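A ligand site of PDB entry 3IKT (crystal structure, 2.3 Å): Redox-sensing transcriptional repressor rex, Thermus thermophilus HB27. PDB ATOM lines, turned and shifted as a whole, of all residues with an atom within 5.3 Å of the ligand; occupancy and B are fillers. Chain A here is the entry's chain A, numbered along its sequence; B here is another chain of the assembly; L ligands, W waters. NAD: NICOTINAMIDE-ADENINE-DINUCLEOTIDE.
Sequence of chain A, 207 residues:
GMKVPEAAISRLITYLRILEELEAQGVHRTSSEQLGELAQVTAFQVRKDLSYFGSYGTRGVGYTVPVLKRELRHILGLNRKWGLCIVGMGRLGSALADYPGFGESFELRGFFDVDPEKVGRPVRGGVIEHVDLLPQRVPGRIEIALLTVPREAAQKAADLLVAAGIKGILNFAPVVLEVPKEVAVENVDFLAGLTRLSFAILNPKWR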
ATOM      1  N   VAL A  87     -16.344   9.293 -10.243  1.00  0.00           N
ATOM      2  CA  VAL A  87     -15.746   8.690 -11.422  1.00  0.00           C
ATOM      3  C   VAL A  87     -14.430   8.079 -10.955  1.00  0.00           C
ATOM      4  O   VAL A  87     -13.497   8.782 -10.563  1.00  0.00           O
ATOM      5  CB  VAL A  87     -15.516   9.723 -12.532  1.00  0.00           C
ATOM      6  CG1 VAL A  87     -14.832   9.083 -13.718  1.00  0.00           C
ATOM      7  CG2 VAL A  87     -16.867  10.318 -12.966  1.00  0.00           C
ATOM      8  N   GLY A  88     -14.368   6.750 -10.997  1.00  0.00           N
ATOM      9  CA  GLY A  88     -13.183   6.027 -10.562  1.00  0.00           C
ATOM     10  C   GLY A  88     -13.543   5.393  -9.226  1.00  0.00           C
ATOM     11  O   GLY A  88     -13.309   5.974  -8.172  1.00  0.00           O
ATOM     12  N   MET A  89     -14.129   4.196  -9.280  1.00  0.00           N
ATOM     13  CA  MET A  89     -14.562   3.512  -8.073  1.00  0.00           C
ATOM     14  C   MET A  89     -13.544   2.558  -7.451  1.00  0.00           C
ATOM     15  O   MET A  89     -13.862   1.393  -7.211  1.00  0.00           O
ATOM     16  CB  MET A  89     -15.871   2.753  -8.327  1.00  0.00           C
ATOM     17  CG  MET A  89     -17.067   3.659  -8.556  1.00  0.00           C
ATOM     18  SD  MET A  89     -17.444   4.692  -7.106  1.00  0.00           S
ATOM     19  CE  MET A  89     -18.156   3.458  -5.993  1.00  0.00           C
ATOM     20  N   GLY A  90     -12.342   3.064  -7.174  1.00  0.00           N
ATOM     21  CA  GLY A  90     -11.328   2.241  -6.544  1.00  0.00           C
ATOM     22  C   GLY A  90     -11.348   2.437  -5.043  1.00  0.00           C
ATOM     23  O   GLY A  90     -12.409   2.650  -4.467  1.00  0.00           O
ATOM     24  N   ARG A  91     -10.194   2.360  -4.394  1.00  0.00           N
ATOM     25  CA  ARG A  91     -10.128   2.541  -2.944  1.00  0.00           C
ATOM     26  C   ARG A  91     -10.702   3.886  -2.487  1.00  0.00           C
ATOM     27  O   ARG A  91     -11.581   3.934  -1.617  1.00  0.00           O
ATOM     28  CB  ARG A  91      -8.678   2.394  -2.448  1.00  0.00           C
ATOM     29  CG  ARG A  91      -8.254   0.949  -2.135  1.00  0.00           C
ATOM     30  CD  ARG A  91      -8.503   0.036  -3.313  1.00  0.00           C
ATOM     31  NE  ARG A  91      -8.512  -1.384  -2.942  1.00  0.00           N
ATOM     32  CZ  ARG A  91      -7.479  -2.042  -2.428  1.00  0.00           C
ATOM     33  NH1 ARG A  91      -6.320  -1.414  -2.238  1.00  0.00           N
ATOM     34  NH2 ARG A  91      -7.590  -3.327  -2.121  1.00  0.00           N
ATOM     35  N   LEU A  92     -10.211   4.975  -3.074  1.00  0.00           N
ATOM     36  CA  LEU A  92     -10.712   6.289  -2.677  1.00  0.00           C
ATOM     37  C   LEU A  92     -12.165   6.461  -3.107  1.00  0.00           C
ATOM     38  O   LEU A  92     -13.003   6.909  -2.321  1.00  0.00           O
ATOM     39  CB  LEU A  92      -9.853   7.399  -3.277  1.00  0.00           C
ATOM     40  CG  LEU A  92     -10.239   8.803  -2.804  1.00  0.00           C
ATOM     41  CD1 LEU A  92     -10.129   8.886  -1.282  1.00  0.00           C
ATOM     42  CD2 LEU A  92      -9.333   9.829  -3.453  1.00  0.00           C
ATOM     43  N   GLY A  93     -12.464   6.107  -4.347  1.00  0.00           N
ATOM     44  CA  GLY A  93     -13.822   6.241  -4.826  1.00  0.00           C
ATOM     45  C   GLY A  93     -14.842   5.539  -3.941  1.00  0.00           C
ATOM     46  O   GLY A  93     -15.892   6.107  -3.611  1.00  0.00           O
ATOM     47  N   PHE A 112     -19.195   5.762 -11.500  1.00  0.00           N
ATOM     48  CA  PHE A 112     -18.698   5.306 -12.781  1.00  0.00           C
ATOM     49  C   PHE A 112     -17.307   4.686 -12.784  1.00  0.00           C
ATOM     50  O   PHE A 112     -16.487   4.954 -11.896  1.00  0.00           O
ATOM     51  CB  PHE A 112     -18.759   6.482 -13.772  1.00  0.00           C
ATOM     52  CG  PHE A 112     -20.139   7.081 -13.910  1.00  0.00           C
ATOM     53  CD1 PHE A 112     -20.647   7.924 -12.919  1.00  0.00           C
ATOM     54  CD2 PHE A 112     -20.966   6.724 -14.977  1.00  0.00           C
ATOM     55  CE1 PHE A 112     -21.962   8.399 -12.994  1.00  0.00           C
ATOM     56  CE2 PHE A 112     -22.287   7.196 -15.058  1.00  0.00           C
ATOM     57  CZ  PHE A 112     -22.781   8.031 -14.061  1.00  0.00           C
ATOM     58  N   ASP A 113     -17.046   3.856 -13.785  1.00  0.00           N
ATOM     59  CA  ASP A 113     -15.757   3.202 -13.927  1.00  0.00           C
ATOM     60  C   ASP A 113     -15.606   2.573 -15.304  1.00  0.00           C
ATOM     61  O   ASP A 113     -16.536   2.630 -16.119  1.00  0.00           O
ATOM     62  CB  ASP A 113     -15.609   2.124 -12.866  1.00  0.00           C
ATOM     63  CG  ASP A 113     -14.167   1.884 -12.496  1.00  0.00           C
ATOM     64  OD1 ASP A 113     -13.740   2.368 -11.436  1.00  0.00           O
ATOM     65  OD2 ASP A 113     -13.450   1.227 -13.283  1.00  0.00           O
ATOM     66  N   VAL A 114     -14.436   2.008 -15.590  1.00  0.00           N
ATOM     67  CA  VAL A 114     -14.209   1.352 -16.875  1.00  0.00           C
ATOM     68  C   VAL A 114     -13.853  -0.102 -16.658  1.00  0.00           C
ATOM     69  O   VAL A 114     -13.779  -0.887 -17.594  1.00  0.00           O
ATOM     70  CB  VAL A 114     -13.056   2.003 -17.670  1.00  0.00           C
ATOM     71  CG1 VAL A 114     -13.402   3.447 -17.987  1.00  0.00           C
ATOM     72  CG2 VAL A 114     -11.748   1.900 -16.887  1.00  0.00           C
ATOM     73  N   ASP A 115     -13.618  -0.459 -15.396  1.00  0.00           N
ATOM     74  CA  ASP A 115     -13.260  -1.829 -15.071  1.00  0.00           C
ATOM     75  C   ASP A 115     -14.458  -2.766 -15.278  1.00  0.00           C
ATOM     76  O   ASP A 115     -15.433  -2.715 -14.543  1.00  0.00           O
ATOM     77  CB  ASP A 115     -12.796  -1.928 -13.620  1.00  0.00           C
ATOM     78  CG  ASP A 115     -12.248  -3.298 -13.279  1.00  0.00           C
ATOM     79  OD1 ASP A 115     -12.483  -4.248 -14.071  1.00  0.00           O
ATOM     80  OD2 ASP A 115     -11.582  -3.434 -12.228  1.00  0.00           O
ATOM     81  N   LYS A 118     -16.143  -4.006 -12.281  1.00  0.00           N
ATOM     82  CA  LYS A 118     -16.759  -3.121 -11.292  1.00  0.00           C
ATOM     83  C   LYS A 118     -18.091  -2.623 -11.819  1.00  0.00           C
ATOM     84  O   LYS A 118     -18.989  -2.319 -11.044  1.00  0.00           O
ATOM     85  CB  LYS A 118     -15.825  -1.961 -10.945  1.00  0.00           C
ATOM     86  CG  LYS A 118     -14.665  -2.398 -10.079  1.00  0.00           C
ATOM     87  CD  LYS A 118     -13.656  -1.307  -9.837  1.00  0.00           C
ATOM     88  CE  LYS A 118     -12.454  -1.857  -9.092  1.00  0.00           C
ATOM     89  NZ  LYS A 118     -11.363  -0.868  -8.911  1.00  0.00           N
ATOM     90  N   VAL A 131     -18.408   4.521 -17.703  1.00  0.00           N
ATOM     91  CA  VAL A 131     -18.323   5.947 -17.984  1.00  0.00           C
ATOM     92  C   VAL A 131     -18.911   6.334 -19.326  1.00  0.00           C
ATOM     93  O   VAL A 131     -19.194   7.500 -19.567  1.00  0.00           O
ATOM     94  CB  VAL A 131     -16.853   6.465 -17.939  1.00  0.00           C
ATOM     95  CG1 VAL A 131     -16.358   6.490 -16.514  1.00  0.00           C
ATOM     96  CG2 VAL A 131     -15.965   5.607 -18.825  1.00  0.00           C
ATOM     97  N   THR A 148     -11.736  10.486  -9.101  1.00  0.00           N
ATOM     98  CA  THR A 148     -10.815   9.629  -8.384  1.00  0.00           C
ATOM     99  C   THR A 148     -10.203   8.473  -9.180  1.00  0.00           C
ATOM    100  O   THR A 148     -10.118   7.351  -8.689  1.00  0.00           O
ATOM    101  CB  THR A 148     -11.496   9.101  -7.096  1.00  0.00           C
ATOM    102  OG1 THR A 148     -12.720   8.429  -7.443  1.00  0.00           O
ATOM    103  CG2 THR A 148     -11.835  10.256  -6.166  1.00  0.00           C
ATOM    104  N   VAL A 149      -9.779   8.760 -10.401  1.00  0.00           N
ATOM    105  CA  VAL A 149      -9.127   7.759 -11.250  1.00  0.00           C
ATOM    106  C   VAL A 149      -7.616   7.994 -11.118  1.00  0.00           C
ATOM    107  O   VAL A 149      -7.199   9.014 -10.575  1.00  0.00           O
ATOM    108  CB  VAL A 149      -9.520   7.914 -12.746  1.00  0.00           C
ATOM    109  CG1 VAL A 149     -11.026   7.751 -12.911  1.00  0.00           C
ATOM    110  CG2 VAL A 149      -9.066   9.266 -13.271  1.00  0.00           C
ATOM    111  N   PRO A 150      -6.784   7.055 -11.613  1.00  0.00           N
ATOM    112  CA  PRO A 150      -5.334   7.245 -11.499  1.00  0.00           C
ATOM    113  C   PRO A 150      -4.880   8.501 -12.237  1.00  0.00           C
ATOM    114  O   PRO A 150      -5.558   8.982 -13.141  1.00  0.00           O
ATOM    115  CB  PRO A 150      -4.765   5.972 -12.134  1.00  0.00           C
ATOM    116  CG  PRO A 150      -5.830   4.951 -11.900  1.00  0.00           C
ATOM    117  CD  PRO A 150      -7.099   5.743 -12.190  1.00  0.00           C
ATOM    118  N   ARG A 151      -3.707   8.995 -11.858  1.00  0.00           N
ATOM    119  CA  ARG A 151      -3.112  10.169 -12.480  1.00  0.00           C
ATOM    120  C   ARG A 151      -3.123  10.130 -14.006  1.00  0.00           C
ATOM    121  O   ARG A 151      -3.553  11.084 -14.645  1.00  0.00           O
ATOM    122  CB  ARG A 151      -1.663  10.316 -11.993  1.00  0.00           C
ATOM    123  CG  ARG A 151      -0.791  11.226 -12.870  1.00  0.00           C
ATOM    124  CD  ARG A 151       0.682  11.097 -12.487  1.00  0.00           C
ATOM    125  NE  ARG A 151       1.166   9.735 -12.664  1.00  0.00           N
ATOM    126  CZ  ARG A 151       1.472   9.193 -13.848  1.00  0.00           C
ATOM    127  NH1 ARG A 151       1.358   9.896 -14.966  1.00  0.00           N
ATOM    128  NH2 ARG A 151       1.893   7.931 -13.905  1.00  0.00           N
ATOM    129  N   ALA A 153      -4.978   8.705 -16.033  1.00  0.00           N
ATOM    130  CA  ALA A 153      -6.307   8.661 -16.629  1.00  0.00           C
ATOM    131  C   ALA A 153      -7.143   9.913 -16.373  1.00  0.00           C
ATOM    132  O   ALA A 153      -8.166  10.114 -17.029  1.00  0.00           O
ATOM    133  CB  ALA A 153      -7.055   7.436 -16.114  1.00  0.00           C
ATOM    134  N   ALA A 157     -10.542  11.396 -18.399  1.00  0.00           N
ATOM    135  CA  ALA A 157     -11.813  11.248 -17.704  1.00  0.00           C
ATOM    136  C   ALA A 157     -12.487  12.620 -17.565  1.00  0.00           C
ATOM    137  O   ALA A 157     -13.705  12.750 -17.687  1.00  0.00           O
ATOM    138  CB  ALA A 157     -11.608  10.619 -16.332  1.00  0.00           C
ATOM    139  N   PHE A 172      -9.166  14.776  -7.379  1.00  0.00           N
ATOM    140  CA  PHE A 172      -8.308  14.155  -6.383  1.00  0.00           C
ATOM    141  C   PHE A 172      -6.991  13.643  -6.967  1.00  0.00           C
ATOM    142  O   PHE A 172      -6.177  13.062  -6.246  1.00  0.00           O
ATOM    143  CB  PHE A 172      -9.026  12.991  -5.698  1.00  0.00           C
ATOM    144  CG  PHE A 172     -10.211  13.395  -4.878  1.00  0.00           C
ATOM    145  CD1 PHE A 172     -11.443  13.663  -5.490  1.00  0.00           C
ATOM    146  CD2 PHE A 172     -10.106  13.523  -3.503  1.00  0.00           C
ATOM    147  CE1 PHE A 172     -12.541  14.053  -4.739  1.00  0.00           C
ATOM    148  CE2 PHE A 172     -11.198  13.924  -2.733  1.00  0.00           C
ATOM    149  CZ  PHE A 172     -12.429  14.185  -3.358  1.00  0.00           C
ATOM    150  N   ALA A 173      -6.788  13.834  -8.273  1.00  0.00           N
ATOM    151  CA  ALA A 173      -5.563  13.362  -8.908  1.00  0.00           C
ATOM    152  C   ALA A 173      -4.505  14.466  -8.930  1.00  0.00           C
ATOM    153  O   ALA A 173      -4.827  15.643  -9.089  1.00  0.00           O
ATOM    154  CB  ALA A 173      -5.847  12.884 -10.330  1.00  0.00           C
ATOM    155  N   PRO A 174      -3.224  14.080  -8.776  1.00  0.00           N
ATOM    156  CA  PRO A 174      -2.099  15.022  -8.762  1.00  0.00           C
ATOM    157  C   PRO A 174      -1.677  15.532 -10.139  1.00  0.00           C
ATOM    158  O   PRO A 174      -0.538  15.385 -10.537  1.00  0.00           O
ATOM    159  CB  PRO A 174      -0.994  14.210  -8.094  1.00  0.00           C
ATOM    160  CG  PRO A 174      -1.259  12.816  -8.615  1.00  0.00           C
ATOM    161  CD  PRO A 174      -2.773  12.711  -8.472  1.00  0.00           C
ATOM    162  N   PHE A 190      -3.753  15.543  -1.544  1.00  0.00           N
ATOM    163  CA  PHE A 190      -3.071  15.175  -0.315  1.00  0.00           C
ATOM    164  C   PHE A 190      -1.556  15.047  -0.466  1.00  0.00           C
ATOM    165  O   PHE A 190      -0.823  15.341   0.470  1.00  0.00           O
ATOM    166  CB  PHE A 190      -3.700  13.929   0.322  1.00  0.00           C
ATOM    167  CG  PHE A 190      -2.929  12.666   0.110  1.00  0.00           C
ATOM    168  CD1 PHE A 190      -3.106  11.902  -1.027  1.00  0.00           C
ATOM    169  CD2 PHE A 190      -2.026  12.226   1.080  1.00  0.00           C
ATOM    170  CE1 PHE A 190      -2.401  10.703  -1.205  1.00  0.00           C
ATOM    171  CE2 PHE A 190      -1.315  11.031   0.909  1.00  0.00           C
ATOM    172  CZ  PHE A 190      -1.512  10.263  -0.235  1.00  0.00           C
ATOM    173  N   LEU A 191      -1.070  14.615  -1.623  1.00  0.00           N
ATOM    174  CA  LEU A 191       0.389  14.506  -1.819  1.00  0.00           C
ATOM    175  C   LEU A 191       1.012  15.893  -1.773  1.00  0.00           C
ATOM    176  O   LEU A 191       2.142  16.060  -1.302  1.00  0.00           O
ATOM    177  CB  LEU A 191       0.724  13.811  -3.135  1.00  0.00           C
ATOM    178  CG  LEU A 191       0.522  12.292  -3.163  1.00  0.00           C
ATOM    179  CD1 LEU A 191       0.600  11.765  -4.600  1.00  0.00           C
ATOM    180  CD2 LEU A 191       1.582  11.623  -2.277  1.00  0.00           C
ATOM    181  N   LEU B  92     -10.748   5.858   5.210  1.00  0.00           N
ATOM    182  CA  LEU B  92      -9.717   6.691   4.601  1.00  0.00           C
ATOM    183  C   LEU B  92      -8.333   6.211   5.014  1.00  0.00           C
ATOM    184  O   LEU B  92      -7.451   6.029   4.171  1.00  0.00           O
ATOM    185  CB  LEU B  92      -9.919   8.165   5.010  1.00  0.00           C
ATOM    186  CG  LEU B  92      -8.909   9.166   4.436  1.00  0.00           C
ATOM    187  CD1 LEU B  92      -8.833   9.013   2.928  1.00  0.00           C
ATOM    188  CD2 LEU B  92      -9.328  10.575   4.816  1.00  0.00           C
ATOM    189  N   ALA B  95      -7.494   3.093   3.384  1.00  0.00           N
ATOM    190  CA  ALA B  95      -7.234   3.338   1.970  1.00  0.00           C
ATOM    191  C   ALA B  95      -5.816   3.879   1.790  1.00  0.00           C
ATOM    192  O   ALA B  95      -5.090   3.500   0.865  1.00  0.00           O
ATOM    193  CB  ALA B  95      -8.262   4.329   1.416  1.00  0.00           C
ATOM    194  N   LEU B  96      -5.412   4.772   2.702  1.00  0.00           N
ATOM    195  CA  LEU B  96      -4.076   5.359   2.648  1.00  0.00           C
ATOM    196  C   LEU B  96      -2.955   4.332   2.869  1.00  0.00           C
ATOM    197  O   LEU B  96      -1.927   4.377   2.181  1.00  0.00           O
ATOM    198  CB  LEU B  96      -3.986   6.497   3.677  1.00  0.00           C
ATOM    199  CG  LEU B  96      -4.763   7.749   3.255  1.00  0.00           C
ATOM    200  CD1 LEU B  96      -4.912   8.743   4.404  1.00  0.00           C
ATOM    201  CD2 LEU B  96      -4.018   8.400   2.080  1.00  0.00           C
ATOM    202  N   ASP B  98      -2.898   1.495   1.950  1.00  0.00           N
ATOM    203  CA  ASP B  98      -2.789   0.744   0.704  1.00  0.00           C
ATOM    204  C   ASP B  98      -2.368   1.596  -0.491  1.00  0.00           C
ATOM    205  O   ASP B  98      -2.086   1.070  -1.563  1.00  0.00           O
ATOM    206  CB  ASP B  98      -4.128   0.072   0.401  1.00  0.00           C
ATOM    207  CG  ASP B  98      -4.452  -1.017   1.392  1.00  0.00           C
ATOM    208  OD1 ASP B  98      -5.631  -1.426   1.475  1.00  0.00           O
ATOM    209  OD2 ASP B  98      -3.514  -1.491   2.076  1.00  0.00           O
ATOM    210  N   TYR B  99      -2.327   2.916  -0.302  1.00  0.00           N
ATOM    211  CA  TYR B  99      -1.945   3.807  -1.383  1.00  0.00           C
ATOM    212  C   TYR B  99      -0.517   3.502  -1.827  1.00  0.00           C
ATOM    213  O   TYR B  99       0.436   3.666  -1.070  1.00  0.00           O
ATOM    214  CB  TYR B  99      -2.084   5.265  -0.922  1.00  0.00           C
ATOM    215  CG  TYR B  99      -1.798   6.272  -1.998  1.00  0.00           C
ATOM    216  CD1 TYR B  99      -2.445   6.203  -3.233  1.00  0.00           C
ATOM    217  CD2 TYR B  99      -0.878   7.304  -1.799  1.00  0.00           C
ATOM    218  CE1 TYR B  99      -2.194   7.123  -4.239  1.00  0.00           C
ATOM    219  CE2 TYR B  99      -0.612   8.224  -2.804  1.00  0.00           C
ATOM    220  CZ  TYR B  99      -1.273   8.128  -4.025  1.00  0.00           C
ATOM    221  OH  TYR B  99      -1.007   9.031  -5.020  1.00  0.00           O
ATOM    222  N   PRO B 100      -0.347   3.049  -3.075  1.00  0.00           N
ATOM    223  CA  PRO B 100       0.978   2.713  -3.611  1.00  0.00           C
ATOM    224  C   PRO B 100       1.706   3.922  -4.175  1.00  0.00           C
ATOM    225  O   PRO B 100       2.642   3.768  -4.950  1.00  0.00           O
ATOM    226  CB  PRO B 100       0.652   1.719  -4.706  1.00  0.00           C
ATOM    227  CG  PRO B 100      -0.598   2.333  -5.294  1.00  0.00           C
ATOM    228  CD  PRO B 100      -1.396   2.722  -4.061  1.00  0.00           C
HETATM  229  PA  NAD L   1      -7.401   2.698  -7.952  1.00  0.00           P
HETATM  230  O1A NAD L   1      -6.597   2.224  -9.049  1.00  0.00           O
HETATM  231  O2A NAD L   1      -7.855   1.948  -6.718  1.00  0.00           O
HETATM  232  O5B NAD L   1      -8.806   3.093  -8.578  1.00  0.00           O
HETATM  233  C5B NAD L   1      -8.877   4.024  -9.700  1.00  0.00           C
HETATM  234  C4B NAD L   1     -10.229   3.527 -10.263  1.00  0.00           C
HETATM  235  O4B NAD L   1     -10.384   4.273 -11.487  1.00  0.00           O
HETATM  236  C3B NAD L   1     -10.068   2.078 -10.769  1.00  0.00           C
HETATM  237  O3B NAD L   1     -11.302   1.465 -10.478  1.00  0.00           O
HETATM  238  C2B NAD L   1      -9.838   2.221 -12.265  1.00  0.00           C
HETATM  239  O2B NAD L   1     -10.347   1.119 -12.992  1.00  0.00           O
HETATM  240  C1B NAD L   1     -10.773   3.436 -12.543  1.00  0.00           C
HETATM  241  N9A NAD L   1     -10.471   4.061 -13.812  1.00  0.00           N
HETATM  242  C8A NAD L   1      -9.315   4.137 -14.593  1.00  0.00           C
HETATM  243  N7A NAD L   1      -9.451   4.840 -15.687  1.00  0.00           N
HETATM  244  C5A NAD L   1     -10.801   5.232 -15.644  1.00  0.00           C
HETATM  245  C6A NAD L   1     -11.531   6.008 -16.552  1.00  0.00           C
HETATM  246  N6A NAD L   1     -11.074   6.569 -17.714  1.00  0.00           N
HETATM  247  N1A NAD L   1     -12.882   6.239 -16.242  1.00  0.00           N
HETATM  248  C2A NAD L   1     -13.462   5.725 -15.055  1.00  0.00           C
HETATM  249  N3A NAD L   1     -12.746   4.957 -14.152  1.00  0.00           N
HETATM  250  C4A NAD L   1     -11.423   4.744 -14.490  1.00  0.00           C
HETATM  251  O3  NAD L   1      -6.812   4.081  -7.379  1.00  0.00           O
HETATM  252  PN  NAD L   1      -6.889   4.827  -5.959  1.00  0.00           P
HETATM  253  O1N NAD L   1      -5.844   4.323  -4.964  1.00  0.00           O
HETATM  254  O2N NAD L   1      -8.289   4.897  -5.505  1.00  0.00           O
HETATM  255  O5D NAD L   1      -6.396   6.267  -6.451  1.00  0.00           O
HETATM  256  C5D NAD L   1      -7.268   7.054  -7.355  1.00  0.00           C
HETATM  257  C4D NAD L   1      -6.847   8.508  -7.225  1.00  0.00           C
HETATM  258  O4D NAD L   1      -6.961   8.859  -5.854  1.00  0.00           O
HETATM  259  C3D NAD L   1      -5.368   8.803  -7.580  1.00  0.00           C
HETATM  260  O3D NAD L   1      -5.233  10.066  -8.296  1.00  0.00           O
HETATM  261  C2D NAD L   1      -4.676   8.957  -6.237  1.00  0.00           C
HETATM  262  O2D NAD L   1      -3.605   9.910  -6.345  1.00  0.00           O
HETATM  263  C1D NAD L   1      -5.733   9.567  -5.421  1.00  0.00           C
HETATM  264  N1N NAD L   1      -5.702   9.233  -3.969  1.00  0.00           N
HETATM  265  C2N NAD L   1      -5.702   7.899  -3.485  1.00  0.00           C
HETATM  266  C3N NAD L   1      -5.686   7.680  -2.115  1.00  0.00           C
HETATM  267  C7N NAD L   1      -5.657   6.262  -1.598  1.00  0.00           C
HETATM  268  O7N NAD L   1      -5.577   6.146  -0.372  1.00  0.00           O
HETATM  269  N7N NAD L   1      -5.657   5.234  -2.394  1.00  0.00           N
HETATM  270  C4N NAD L   1      -5.693   8.798  -1.158  1.00  0.00           C
HETATM  271  C5N NAD L   1      -5.733  10.127  -1.691  1.00  0.00           C
HETATM  272  C6N NAD L   1      -5.671  10.364  -3.092  1.00  0.00           C
HETATM  273  O   HOH W   1      -2.615   8.039  -9.028  1.00  0.00           O
HETATM  274  O   HOH W   2     -10.855   5.395  -6.550  1.00  0.00           O
HETATM  275  O   HOH W   3      -5.406   2.781  -1.583  1.00  0.00           O
HETATM  276  O   HOH W   4      -6.678   1.397 -11.718  1.00  0.00           O
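OD1 of Asp 113 is in hydrogen-bond range of O3B of the ligand, 2.8 Å away.
The side-chain amino group (NZ) of Lys 118 lies within hydrogen-bond range of an oxygen (O3B) of the ligand, at 2.8 Å.
The backbone NH (N) of Leu 92 of chain A sits at hydrogen-bond distance from an oxygen (O2N) of the ligand (3.1 Å).
N of Leu 96 of chain B lies within hydrogen-bond range of O7N of the ligand, 3.4 Å away.
The backbone NH (N) of Arg 91 lies within hydrogen-bond range of an oxygen (O2A) of the ligand, 3.3 Å away.
The side-chain hydroxyl of Tyr 99 of chain B is in hydrogen-bond range of an oxygen (O2D) of the ligand (3.0 Å).
O3D of the ligand lies within hydrogen-bond range of O of Val 149, at 3.2 Å.
Water W3 lies within hydrogen-bond range of the backbone carbonyl oxygen of Ala 95 of chain B (2.6 Å), a nitrogen (N7N) of the ligand (2.6 Å) and the backbone NH of Tyr 99 of chain B (3.3 Å).
Water W2 lies within hydrogen-bond range of an oxygen (O2N) of the ligand, the backbone NH (N) of Gly 93, the backbone NH (N) of Gly 90, the backbone carbonyl oxygen (O) of Thr 148 and the backbone carbonyl oxygen (O) of Gly 88.
Water W1 lies within hydrogen-bond range of N of Arg 151 (3.2 Å) and O3D of the ligand (3.4 Å).
The backbone carbonyl oxygen of Ala 95 of chain B sits close to an oxygen (O7N) of the ligand (3.0 Å).
Residues that only touch the ligand: Val 87, Gly 88, Met 89, Gly 90, Val 114, Asp 115, Val 131, Thr 148, Pro 150, Ala 153, Phe 172, Ala 173, Pro 174 and Phe 190.
Hydrophobic or aromatic side chains within 4 Å of the ligand: Val 87, Leu 92 of chain A, Val 114, Val 131, Val 149, Pro 150, Ala 153, Ala 173, Pro 174, Phe 190, Ala 95 of chain B, Leu 96 of chain B and Tyr 99 of chain B.
Within 4 Å of the ligand: Val 87, Gly 88, Met 89, Gly 90, Arg 91, Leu 92 of chain A, Asp 113, Val 114, Asp 115, Lys 118, Val 131, Thr 148, Val 149, Pro 150, Ala 153, Phe 172, Ala 173, Pro 174, Phe 190, Ala 95 of chain B, Leu 96 of chain B and Tyr 99 of chain B.
The nearest printed residue that does not touch the ligand is Arg 151 (4.02 Å).
The backbone carbonyl oxygen of Asp 113 is in hydrogen-bond range of the backbone NH of Val 131, 3.1 Å away.
OD2 of Asp 113 is in hydrogen-bond range of N of Asp 115.
The backbone NH of Met 89 lies within hydrogen-bond range of the side-chain carboxylate of Asp 113 (2.9 Å).
N of Thr 148 is in hydrogen-bond range of O of Val 87 (2.9 Å).
The side-chain carboxylate of Asp 98 of chain B is in salt-bridge range of the guanidinium group of Arg 91 (3.8 Å).
O of Gly 88 sits at hydrogen-bond distance from OG1 of Thr 148 (2.6 Å).
The backbone NH (N) of Gly 88 is in hydrogen-bond range of the backbone carbonyl oxygen (O) of Phe 112 (2.9 Å).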
